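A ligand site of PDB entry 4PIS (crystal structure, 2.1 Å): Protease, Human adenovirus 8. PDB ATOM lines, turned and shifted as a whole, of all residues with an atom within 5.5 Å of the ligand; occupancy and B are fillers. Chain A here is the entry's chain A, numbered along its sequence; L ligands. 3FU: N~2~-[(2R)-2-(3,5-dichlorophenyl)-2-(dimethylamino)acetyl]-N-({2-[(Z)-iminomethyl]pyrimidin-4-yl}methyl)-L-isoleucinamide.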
ATOM      1  N   SER A   1      33.281 -14.860   4.486  1.00  0.00           N
ATOM      2  CA  SER A   1      33.699 -13.476   4.363  1.00  0.00           C
ATOM      3  C   SER A   1      32.779 -12.571   5.190  1.00  0.00           C
ATOM      4  O   SER A   1      31.638 -12.295   4.794  1.00  0.00           O
ATOM      5  CB  SER A   1      33.718 -13.051   2.889  1.00  0.00           C
ATOM      6  OG  SER A   1      34.016 -11.677   2.712  1.00  0.00           O
ATOM      7  N   GLY A   2      33.296 -12.127   6.330  1.00  0.00           N
ATOM      8  CA  GLY A   2      32.557 -11.261   7.235  1.00  0.00           C
ATOM      9  C   GLY A   2      31.775 -11.997   8.302  1.00  0.00           C
ATOM     10  O   GLY A   2      31.863 -13.231   8.429  1.00  0.00           O
ATOM     11  N   SER A   3      31.010 -11.232   9.066  1.00  0.00           N
ATOM     12  CA  SER A   3      30.196 -11.710  10.183  1.00  0.00           C
ATOM     13  C   SER A   3      28.770 -11.964   9.716  1.00  0.00           C
ATOM     14  O   SER A   3      28.232 -11.171   8.929  1.00  0.00           O
ATOM     15  CB  SER A   3      30.185 -10.675  11.312  1.00  0.00           C
ATOM     16  OG  SER A   3      31.481 -10.204  11.625  1.00  0.00           O
ATOM     17  N   SER A   4      28.182 -13.079  10.203  1.00  0.00           N
ATOM     18  CA  SER A   4      26.800 -13.510   9.924  1.00  0.00           C
ATOM     19  C   SER A   4      25.841 -12.733  10.835  1.00  0.00           C
ATOM     20  O   SER A   4      26.290 -12.193  11.838  1.00  0.00           O
ATOM     21  CB  SER A   4      26.664 -15.014  10.177  1.00  0.00           C
ATOM     22  OG  SER A   4      26.825 -15.337  11.553  1.00  0.00           O
ATOM     23  N   GLU A   5      24.546 -12.718  10.551  1.00  0.00           N
ATOM     24  CA  GLU A   5      23.585 -12.011  11.409  1.00  0.00           C
ATOM     25  C   GLU A   5      23.456 -12.603  12.831  1.00  0.00           C
ATOM     26  O   GLU A   5      23.155 -11.866  13.775  1.00  0.00           O
ATOM     27  CB  GLU A   5      22.216 -11.883  10.727  1.00  0.00           C
ATOM     28  CG  GLU A   5      21.445 -13.186  10.587  1.00  0.00           C
ATOM     29  CD  GLU A   5      20.001 -13.019  10.168  1.00  0.00           C
ATOM     30  OE1 GLU A   5      19.635 -13.561   9.107  1.00  0.00           O
ATOM     31  OE2 GLU A   5      19.229 -12.360  10.908  1.00  0.00           O
ATOM     32  N   GLN A   6      23.725 -13.917  12.989  1.00  0.00           N
ATOM     33  CA  GLN A   6      23.645 -14.627  14.282  1.00  0.00           C
ATOM     34  C   GLN A   6      24.838 -14.216  15.132  1.00  0.00           C
ATOM     35  O   GLN A   6      24.711 -14.032  16.341  1.00  0.00           O
ATOM     36  CB  GLN A   6      23.666 -16.166  14.087  1.00  0.00           C
ATOM     37  CG  GLN A   6      22.587 -16.716  13.139  1.00  0.00           C
ATOM     38  CD  GLN A   6      22.913 -16.576  11.656  1.00  0.00           C
ATOM     39  OE1 GLN A   6      24.069 -16.494  11.255  1.00  0.00           O
ATOM     40  NE2 GLN A   6      21.885 -16.549  10.816  1.00  0.00           N
ATOM     41  N   THR A  24      19.135  -7.343  13.130  1.00  0.00           N
ATOM     42  CA  THR A  24      20.032  -7.273  11.979  1.00  0.00           C
ATOM     43  C   THR A  24      19.183  -7.476  10.733  1.00  0.00           C
ATOM     44  O   THR A  24      18.366  -8.408  10.691  1.00  0.00           O
ATOM     45  CB  THR A  24      21.192  -8.281  12.106  1.00  0.00           C
ATOM     46  OG1 THR A  24      20.637  -9.573  12.365  1.00  0.00           O
ATOM     47  CG2 THR A  24      22.146  -7.948  13.243  1.00  0.00           C
ATOM     48  N   HIS A  25      19.325  -6.554   9.765  1.00  0.00           N
ATOM     49  CA  HIS A  25      18.506  -6.572   8.550  1.00  0.00           C
ATOM     50  C   HIS A  25      19.351  -6.337   7.319  1.00  0.00           C
ATOM     51  O   HIS A  25      20.542  -6.058   7.419  1.00  0.00           O
ATOM     52  CB  HIS A  25      17.471  -5.416   8.603  1.00  0.00           C
ATOM     53  CG  HIS A  25      16.638  -5.376   9.840  1.00  0.00           C
ATOM     54  ND1 HIS A  25      15.312  -5.725   9.821  1.00  0.00           N
ATOM     55  CD2 HIS A  25      16.977  -4.986  11.089  1.00  0.00           C
ATOM     56  CE1 HIS A  25      14.881  -5.557  11.055  1.00  0.00           C
ATOM     57  NE2 HIS A  25      15.853  -5.111  11.860  1.00  0.00           N
ATOM     58  N   ASP A  26      18.695  -6.389   6.169  1.00  0.00           N
ATOM     59  CA  ASP A  26      19.249  -6.080   4.872  1.00  0.00           C
ATOM     60  C   ASP A  26      18.848  -4.616   4.591  1.00  0.00           C
ATOM     61  O   ASP A  26      18.156  -4.032   5.409  1.00  0.00           O
ATOM     62  CB  ASP A  26      18.696  -7.074   3.822  1.00  0.00           C
ATOM     63  CG  ASP A  26      17.218  -6.998   3.457  1.00  0.00           C
ATOM     64  OD1 ASP A  26      16.490  -6.184   4.083  1.00  0.00           O
ATOM     65  OD2 ASP A  26      16.794  -7.724   2.545  1.00  0.00           O
ATOM     66  N   LYS A  27      19.248  -4.060   3.432  1.00  0.00           N
ATOM     67  CA  LYS A  27      18.960  -2.683   2.995  1.00  0.00           C
ATOM     68  C   LYS A  27      17.495  -2.199   3.197  1.00  0.00           C
ATOM     69  O   LYS A  27      17.257  -0.985   3.255  1.00  0.00           O
ATOM     70  CB  LYS A  27      19.383  -2.501   1.527  1.00  0.00           C
ATOM     71  CG  LYS A  27      18.574  -3.300   0.506  1.00  0.00           C
ATOM     72  CD  LYS A  27      18.910  -2.869  -0.908  1.00  0.00           C
ATOM     73  CE  LYS A  27      18.094  -3.614  -1.935  1.00  0.00           C
ATOM     74  NZ  LYS A  27      18.516  -3.275  -3.327  1.00  0.00           N
ATOM     75  N   ASN A  44      22.416  -4.223   6.434  1.00  0.00           N
ATOM     76  CA  ASN A  44      23.313  -4.537   5.350  1.00  0.00           C
ATOM     77  C   ASN A  44      23.045  -3.588   4.194  1.00  0.00           C
ATOM     78  O   ASN A  44      21.884  -3.238   3.980  1.00  0.00           O
ATOM     79  CB  ASN A  44      23.148  -5.987   4.905  1.00  0.00           C
ATOM     80  CG  ASN A  44      24.362  -6.508   4.153  1.00  0.00           C
ATOM     81  OD1 ASN A  44      24.516  -6.295   2.948  1.00  0.00           O
ATOM     82  ND2 ASN A  44      25.268  -7.154   4.855  1.00  0.00           N
ATOM     83  N   ALA A  46      23.163  -4.385   1.107  1.00  0.00           N
ATOM     84  CA  ALA A  46      22.472  -5.148   0.076  1.00  0.00           C
ATOM     85  C   ALA A  46      21.193  -5.864   0.547  1.00  0.00           C
ATOM     86  O   ALA A  46      20.905  -5.890   1.733  1.00  0.00           O
ATOM     87  CB  ALA A  46      23.455  -6.136  -0.538  1.00  0.00           C
ATOM     88  N   GLY A  47      20.425  -6.396  -0.394  1.00  0.00           N
ATOM     89  CA  GLY A  47      19.223  -7.191  -0.104  1.00  0.00           C
ATOM     90  C   GLY A  47      19.634  -8.607   0.242  1.00  0.00           C
ATOM     91  O   GLY A  47      20.616  -9.102  -0.327  1.00  0.00           O
ATOM     92  N   ARG A  48      18.907  -9.285   1.165  1.00  0.00           N
ATOM     93  CA  ARG A  48      19.192 -10.660   1.639  1.00  0.00           C
ATOM     94  C   ARG A  48      19.490 -11.685   0.517  1.00  0.00           C
ATOM     95  O   ARG A  48      20.300 -12.604   0.721  1.00  0.00           O
ATOM     96  CB  ARG A  48      18.065 -11.186   2.554  1.00  0.00           C
ATOM     97  CG  ARG A  48      18.393 -12.527   3.236  1.00  0.00           C
ATOM     98  CD  ARG A  48      17.296 -13.018   4.167  1.00  0.00           C
ATOM     99  NE  ARG A  48      17.296 -12.291   5.433  1.00  0.00           N
ATOM    100  CZ  ARG A  48      18.016 -12.633   6.493  1.00  0.00           C
ATOM    101  NH1 ARG A  48      17.968 -11.920   7.606  1.00  0.00           N
ATOM    102  NH2 ARG A  48      18.809 -13.711   6.443  1.00  0.00           N
ATOM    103  N   THR A  50      20.974 -11.182  -2.363  1.00  0.00           N
ATOM    104  CA  THR A  50      22.295 -11.056  -2.961  1.00  0.00           C
ATOM    105  C   THR A  50      23.327 -11.807  -2.099  1.00  0.00           C
ATOM    106  O   THR A  50      24.397 -12.149  -2.596  1.00  0.00           O
ATOM    107  CB  THR A  50      22.676  -9.596  -3.186  1.00  0.00           C
ATOM    108  OG1 THR A  50      22.780  -8.945  -1.927  1.00  0.00           O
ATOM    109  CG2 THR A  50      21.701  -8.876  -4.112  1.00  0.00           C
ATOM    110  N   GLY A  51      22.969 -12.031  -0.831  1.00  0.00           N
ATOM    111  CA  GLY A  51      23.781 -12.752   0.151  1.00  0.00           C
ATOM    112  C   GLY A  51      24.524 -11.915   1.160  1.00  0.00           C
ATOM    113  O   GLY A  51      25.193 -12.461   2.043  1.00  0.00           O
ATOM    114  N   GLY A  52      24.407 -10.581   1.052  1.00  0.00           N
ATOM    115  CA  GLY A  52      25.079  -9.640   1.940  1.00  0.00           C
ATOM    116  C   GLY A  52      26.409  -9.148   1.395  1.00  0.00           C
ATOM    117  O   GLY A  52      27.169  -9.911   0.811  1.00  0.00           O
ATOM    118  N   VAL A  53      26.680  -7.832   1.582  1.00  0.00           N
ATOM    119  CA  VAL A  53      27.881  -7.178   1.045  1.00  0.00           C
ATOM    120  C   VAL A  53      28.629  -6.382   2.100  1.00  0.00           C
ATOM    121  O   VAL A  53      29.840  -6.540   2.217  1.00  0.00           O
ATOM    122  CB  VAL A  53      27.489  -6.299  -0.176  1.00  0.00           C
ATOM    123  CG1 VAL A  53      28.629  -5.377  -0.610  1.00  0.00           C
ATOM    124  CG2 VAL A  53      26.989  -7.137  -1.345  1.00  0.00           C
ATOM    125  N   HIS A  54      27.933  -5.477   2.814  1.00  0.00           N
ATOM    126  CA  HIS A  54      28.613  -4.619   3.793  1.00  0.00           C
ATOM    127  C   HIS A  54      27.730  -4.324   5.007  1.00  0.00           C
ATOM    128  O   HIS A  54      26.533  -4.215   4.869  1.00  0.00           O
ATOM    129  CB  HIS A  54      29.066  -3.332   3.074  1.00  0.00           C
ATOM    130  CG  HIS A  54      29.784  -2.336   3.927  1.00  0.00           C
ATOM    131  ND1 HIS A  54      30.928  -2.670   4.635  1.00  0.00           N
ATOM    132  CD2 HIS A  54      29.540  -1.016   4.109  1.00  0.00           C
ATOM    133  CE1 HIS A  54      31.301  -1.571   5.261  1.00  0.00           C
ATOM    134  NE2 HIS A  54      30.494  -0.554   4.986  1.00  0.00           N
ATOM    135  N   TRP A  55      28.314  -4.149   6.181  1.00  0.00           N
ATOM    136  CA  TRP A  55      27.506  -3.853   7.365  1.00  0.00           C
ATOM    137  C   TRP A  55      27.565  -2.398   7.823  1.00  0.00           C
ATOM    138  O   TRP A  55      28.642  -1.807   7.891  1.00  0.00           O
ATOM    139  CB  TRP A  55      27.839  -4.789   8.535  1.00  0.00           C
ATOM    140  CG  TRP A  55      27.492  -6.223   8.301  1.00  0.00           C
ATOM    141  CD1 TRP A  55      28.367  -7.260   8.134  1.00  0.00           C
ATOM    142  CD2 TRP A  55      26.170  -6.804   8.267  1.00  0.00           C
ATOM    143  NE1 TRP A  55      27.685  -8.442   8.022  1.00  0.00           N
ATOM    144  CE2 TRP A  55      26.337  -8.192   8.040  1.00  0.00           C
ATOM    145  CE3 TRP A  55      24.867  -6.280   8.330  1.00  0.00           C
ATOM    146  CZ2 TRP A  55      25.244  -9.065   7.956  1.00  0.00           C
ATOM    147  CZ3 TRP A  55      23.790  -7.147   8.215  1.00  0.00           C
ATOM    148  CH2 TRP A  55      23.982  -8.526   8.035  1.00  0.00           C
ATOM    149  N   PHE A  73      33.867   2.593   7.387  1.00  0.00           N
ATOM    150  CA  PHE A  73      34.643   3.227   6.320  1.00  0.00           C
ATOM    151  C   PHE A  73      34.395   4.752   6.180  1.00  0.00           C
ATOM    152  O   PHE A  73      35.091   5.389   5.405  1.00  0.00           O
ATOM    153  CB  PHE A  73      34.292   2.550   4.980  1.00  0.00           C
ATOM    154  CG  PHE A  73      34.885   1.167   4.741  1.00  0.00           C
ATOM    155  CD1 PHE A  73      34.180   0.223   4.023  1.00  0.00           C
ATOM    156  CD2 PHE A  73      36.161   0.860   5.194  1.00  0.00           C
ATOM    157  CE1 PHE A  73      34.747  -1.027   3.749  1.00  0.00           C
ATOM    158  CE2 PHE A  73      36.728  -0.390   4.920  1.00  0.00           C
ATOM    159  CZ  PHE A  73      36.019  -1.323   4.196  1.00  0.00           C
ATOM    160  N   GLN A 115      38.428   1.265   9.526  1.00  0.00           N
ATOM    161  CA  GLN A 115      38.700   0.010   8.899  1.00  0.00           C
ATOM    162  C   GLN A 115      39.640   0.077   7.700  1.00  0.00           C
ATOM    163  O   GLN A 115      39.480   0.954   6.841  1.00  0.00           O
ATOM    164  CB  GLN A 115      37.360  -0.601   8.492  1.00  0.00           C
ATOM    165  CG  GLN A 115      37.414  -2.084   8.174  1.00  0.00           C
ATOM    166  CD  GLN A 115      36.065  -2.626   7.778  1.00  0.00           C
ATOM    167  OE1 GLN A 115      35.927  -3.480   6.897  1.00  0.00           O
ATOM    168  NE2 GLN A 115      35.051  -2.138   8.434  1.00  0.00           N
ATOM    169  N   SER A 119      39.886  -5.301   4.926  1.00  0.00           N
ATOM    170  CA  SER A 119      39.291  -5.909   6.099  1.00  0.00           C
ATOM    171  C   SER A 119      37.817  -6.282   5.909  1.00  0.00           C
ATOM    172  O   SER A 119      37.089  -5.668   5.112  1.00  0.00           O
ATOM    173  CB  SER A 119      39.513  -5.034   7.326  1.00  0.00           C
ATOM    174  OG  SER A 119      38.678  -5.448   8.390  1.00  0.00           O
ATOM    175  N   ALA A 120      37.397  -7.330   6.649  1.00  0.00           N
ATOM    176  CA  ALA A 120      36.032  -7.843   6.644  1.00  0.00           C
ATOM    177  C   ALA A 120      35.444  -7.817   8.059  1.00  0.00           C
ATOM    178  O   ALA A 120      34.506  -8.549   8.358  1.00  0.00           O
ATOM    179  CB  ALA A 120      36.006  -9.248   6.040  1.00  0.00           C
ATOM    180  N   ALA A 121      35.965  -6.897   8.896  1.00  0.00           N
ATOM    181  CA  ALA A 121      35.534  -6.656  10.266  1.00  0.00           C
ATOM    182  C   ALA A 121      34.419  -5.610  10.370  1.00  0.00           C
ATOM    183  O   ALA A 121      34.101  -5.251  11.496  1.00  0.00           O
ATOM    184  CB  ALA A 121      36.730  -6.272  11.141  1.00  0.00           C
ATOM    185  N   CYS A 122      33.773  -5.176   9.246  1.00  0.00           N
ATOM    186  CA  CYS A 122      32.701  -4.149   9.239  1.00  0.00           C
ATOM    187  C   CYS A 122      31.571  -4.411  10.259  1.00  0.00           C
ATOM    188  O   CYS A 122      31.245  -3.511  11.024  1.00  0.00           O
ATOM    189  CB  CYS A 122      32.137  -3.869   7.853  1.00  0.00           C
ATOM    190  SG  CYS A 122      31.356  -5.288   7.033  1.00  0.00           S
ATOM    191  N   GLY A 123      31.037  -5.629  10.268  1.00  0.00           N
ATOM    192  CA  GLY A 123      30.015  -6.067  11.217  1.00  0.00           C
ATOM    193  C   GLY A 123      30.470  -5.930  12.653  1.00  0.00           C
ATOM    194  O   GLY A 123      29.714  -5.473  13.509  1.00  0.00           O
ATOM    195  N   MET A 201      39.861  -9.491   2.104  1.00  0.00           N
ATOM    196  CA  MET A 201      39.407  -9.251   0.729  1.00  0.00           C
ATOM    197  C   MET A 201      40.453  -9.654  -0.321  1.00  0.00           C
ATOM    198  O   MET A 201      40.089 -10.029  -1.447  1.00  0.00           O
ATOM    199  CB  MET A 201      38.890  -7.823   0.504  1.00  0.00           C
ATOM    200  CG  MET A 201      37.640  -7.462   1.340  1.00  0.00           C
ATOM    201  SD  MET A 201      36.404  -8.792   1.558  1.00  0.00           S
ATOM    202  CE  MET A 201      35.658  -8.813  -0.131  1.00  0.00           C
HETATM  203  C11 3FU L   1      21.057 -10.257   6.616  1.00  0.00           C
HETATM  204  C12 3FU L   1      21.105  -9.381   5.512  1.00  0.00           C
HETATM  205  C13 3FU L   1      21.878  -9.708   4.387  1.00  0.00           C
HETATM  206  C14 3FU L   1      22.620 -10.925   4.376  1.00  0.00           C
HETATM  207  C22 3FU L   1      23.896 -15.318   4.555  1.00  0.00           C
HETATM  208  C23 3FU L   1      22.000 -14.102   3.660  1.00  0.00           C
HETATM  209  C7  3FU L   1      24.667 -12.722   6.142  1.00  0.00           C
HETATM  210  C8  3FU L   1      23.301 -13.142   5.622  1.00  0.00           C
HETATM  211  C9  3FU L   1      22.569 -11.794   5.496  1.00  0.00           C
HETATM  212  C10 3FU L   1      21.783 -11.440   6.600  1.00  0.00           C
HETATM  213 CL1  3FU L   1      20.180  -9.893   8.078  1.00  0.00          CL
HETATM  214 CL2  3FU L   1      21.892  -8.643   2.987  1.00  0.00          CL
HETATM  215  O17 3FU L   1      24.795 -12.721   7.361  1.00  0.00           O
HETATM  216  N21 3FU L   1      23.322 -13.951   4.346  1.00  0.00           N
HETATM  217  N3  3FU L   1      25.651 -12.368   5.262  1.00  0.00           N
HETATM  218  C2  3FU L   1      27.012 -11.928   5.648  1.00  0.00           C
HETATM  219  C1  3FU L   1      27.292 -10.509   5.129  1.00  0.00           C
HETATM  220  O4  3FU L   1      26.363  -9.846   4.679  1.00  0.00           O
HETATM  221  C5  3FU L   1      28.132 -12.945   5.221  1.00  0.00           C
HETATM  222  C18 3FU L   1      28.043 -13.477   3.749  1.00  0.00           C
HETATM  223  C20 3FU L   1      28.183 -14.124   6.227  1.00  0.00           C
HETATM  224  C19 3FU L   1      28.703 -12.584   2.660  1.00  0.00           C
HETATM  225  C24 3FU L   1      28.833  -8.667   4.684  1.00  0.00           C
HETATM  226  C25 3FU L   1      30.346  -8.435   4.617  1.00  0.00           C
HETATM  227  C27 3FU L   1      32.204  -7.146   5.332  1.00  0.00           C
HETATM  228  C29 3FU L   1      32.557  -8.935   3.795  1.00  0.00           C
HETATM  229  C30 3FU L   1      31.174  -9.214   3.802  1.00  0.00           C
HETATM  230  N6  3FU L   1      28.553 -10.001   5.191  1.00  0.00           N
HETATM  231  N26 3FU L   1      30.867  -7.418   5.339  1.00  0.00           N
HETATM  232  N28 3FU L   1      33.041  -7.917   4.573  1.00  0.00           N
HETATM  233  C31 3FU L   1      32.742  -6.040   6.114  1.00  0.00           C
HETATM  234  N32 3FU L   1      33.742  -5.307   5.698  1.00  0.00           N
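N26 of the ligand lies close to O of Val 53 (3.4 Å).
The backbone carbonyl oxygen of Gly 51 lies within hydrogen-bond range of a nitrogen (N3) of the ligand, 3.3 Å away.
C31 of the ligand is bonded to SG of Cys 122, at 1.8 Å.
The side-chain amide oxygen of Gln 115 sits at hydrogen-bond distance from a nitrogen (N32) of the ligand (3.1 Å).
The backbone carbonyl oxygen of Ser 119 is in hydrogen-bond range of a nitrogen (N32) of the ligand, 3.4 Å away.
The side-chain amide nitrogen (ND2) of Asn 44 is in hydrogen-bond range of an oxygen (O4) of the ligand (2.9 Å).
The backbone NH (N) of Glu 5 sits at hydrogen-bond distance from an oxygen (O17) of the ligand, 3.2 Å away.
OG of Ser 4 lies within hydrogen-bond range of OE1 of Gln 6 (3.0 Å).
The side-chain hydroxyl (OG1) of Thr 24 sits close to the side-chain carboxylate (OE2) of Glu 5.
The indole nitrogen of Trp 55 is in hydrogen-bond range of the backbone carbonyl oxygen of Ser 3 (2.9 Å).
A ring nitrogen (ND1) of His 54 is in hydrogen-bond range of the side-chain sulfur (SG) of Cys 122 (3.6 Å).
The backbone NH (N) of Val 53 is in hydrogen-bond range of the side-chain amide oxygen (OD1) of Asn 44.
The side-chain amide oxygen (OD1) of Asn 44 is in hydrogen-bond range of the backbone NH (N) of Ala 46, at 3.0 Å.
The backbone NH of Arg 48 sits at hydrogen-bond distance from the side-chain carboxylate of Asp 26.
ND2 of Asn 44 is in hydrogen-bond range of O of His 54.
The indole nitrogen of Trp 55 sits close to a nitrogen (N6) of the ligand, at 3.3 Å.
Ser 1 touches the ligand (O to C30, 3.3 Å).
Ser 3 touches the ligand (O to C2, 3.6 Å).
Ser 4 touches the ligand (CA to O17, 3.3 Å).
Thr 24 touches the ligand (O to CL1, 3.5 Å).
His 25 touches the ligand.
Asp 26 touches the ligand.
O of Ala 46 touches CL2 of the ligand (3.2 Å).
Gly 47 touches the ligand (C to CL2, 3.6 Å).
NH1 of Arg 48 touches CL1 of the ligand, 3.0 Å away.
Gly 52 touches the ligand (CA to O4, 3.0 Å).
N of His 54 touches C24 of the ligand, at 3.8 Å.
Ala 120 touches the ligand (CA to N32, 3.5 Å).
Hydrophobic or aromatic side chains within 4 Å of the ligand: Trp 55 and Ala 120.
Of the 28 residues printed, 20 come within 4 Å of the ligand.
Along chain A the residues within 4 Å of the ligand span positions 1 to 122.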
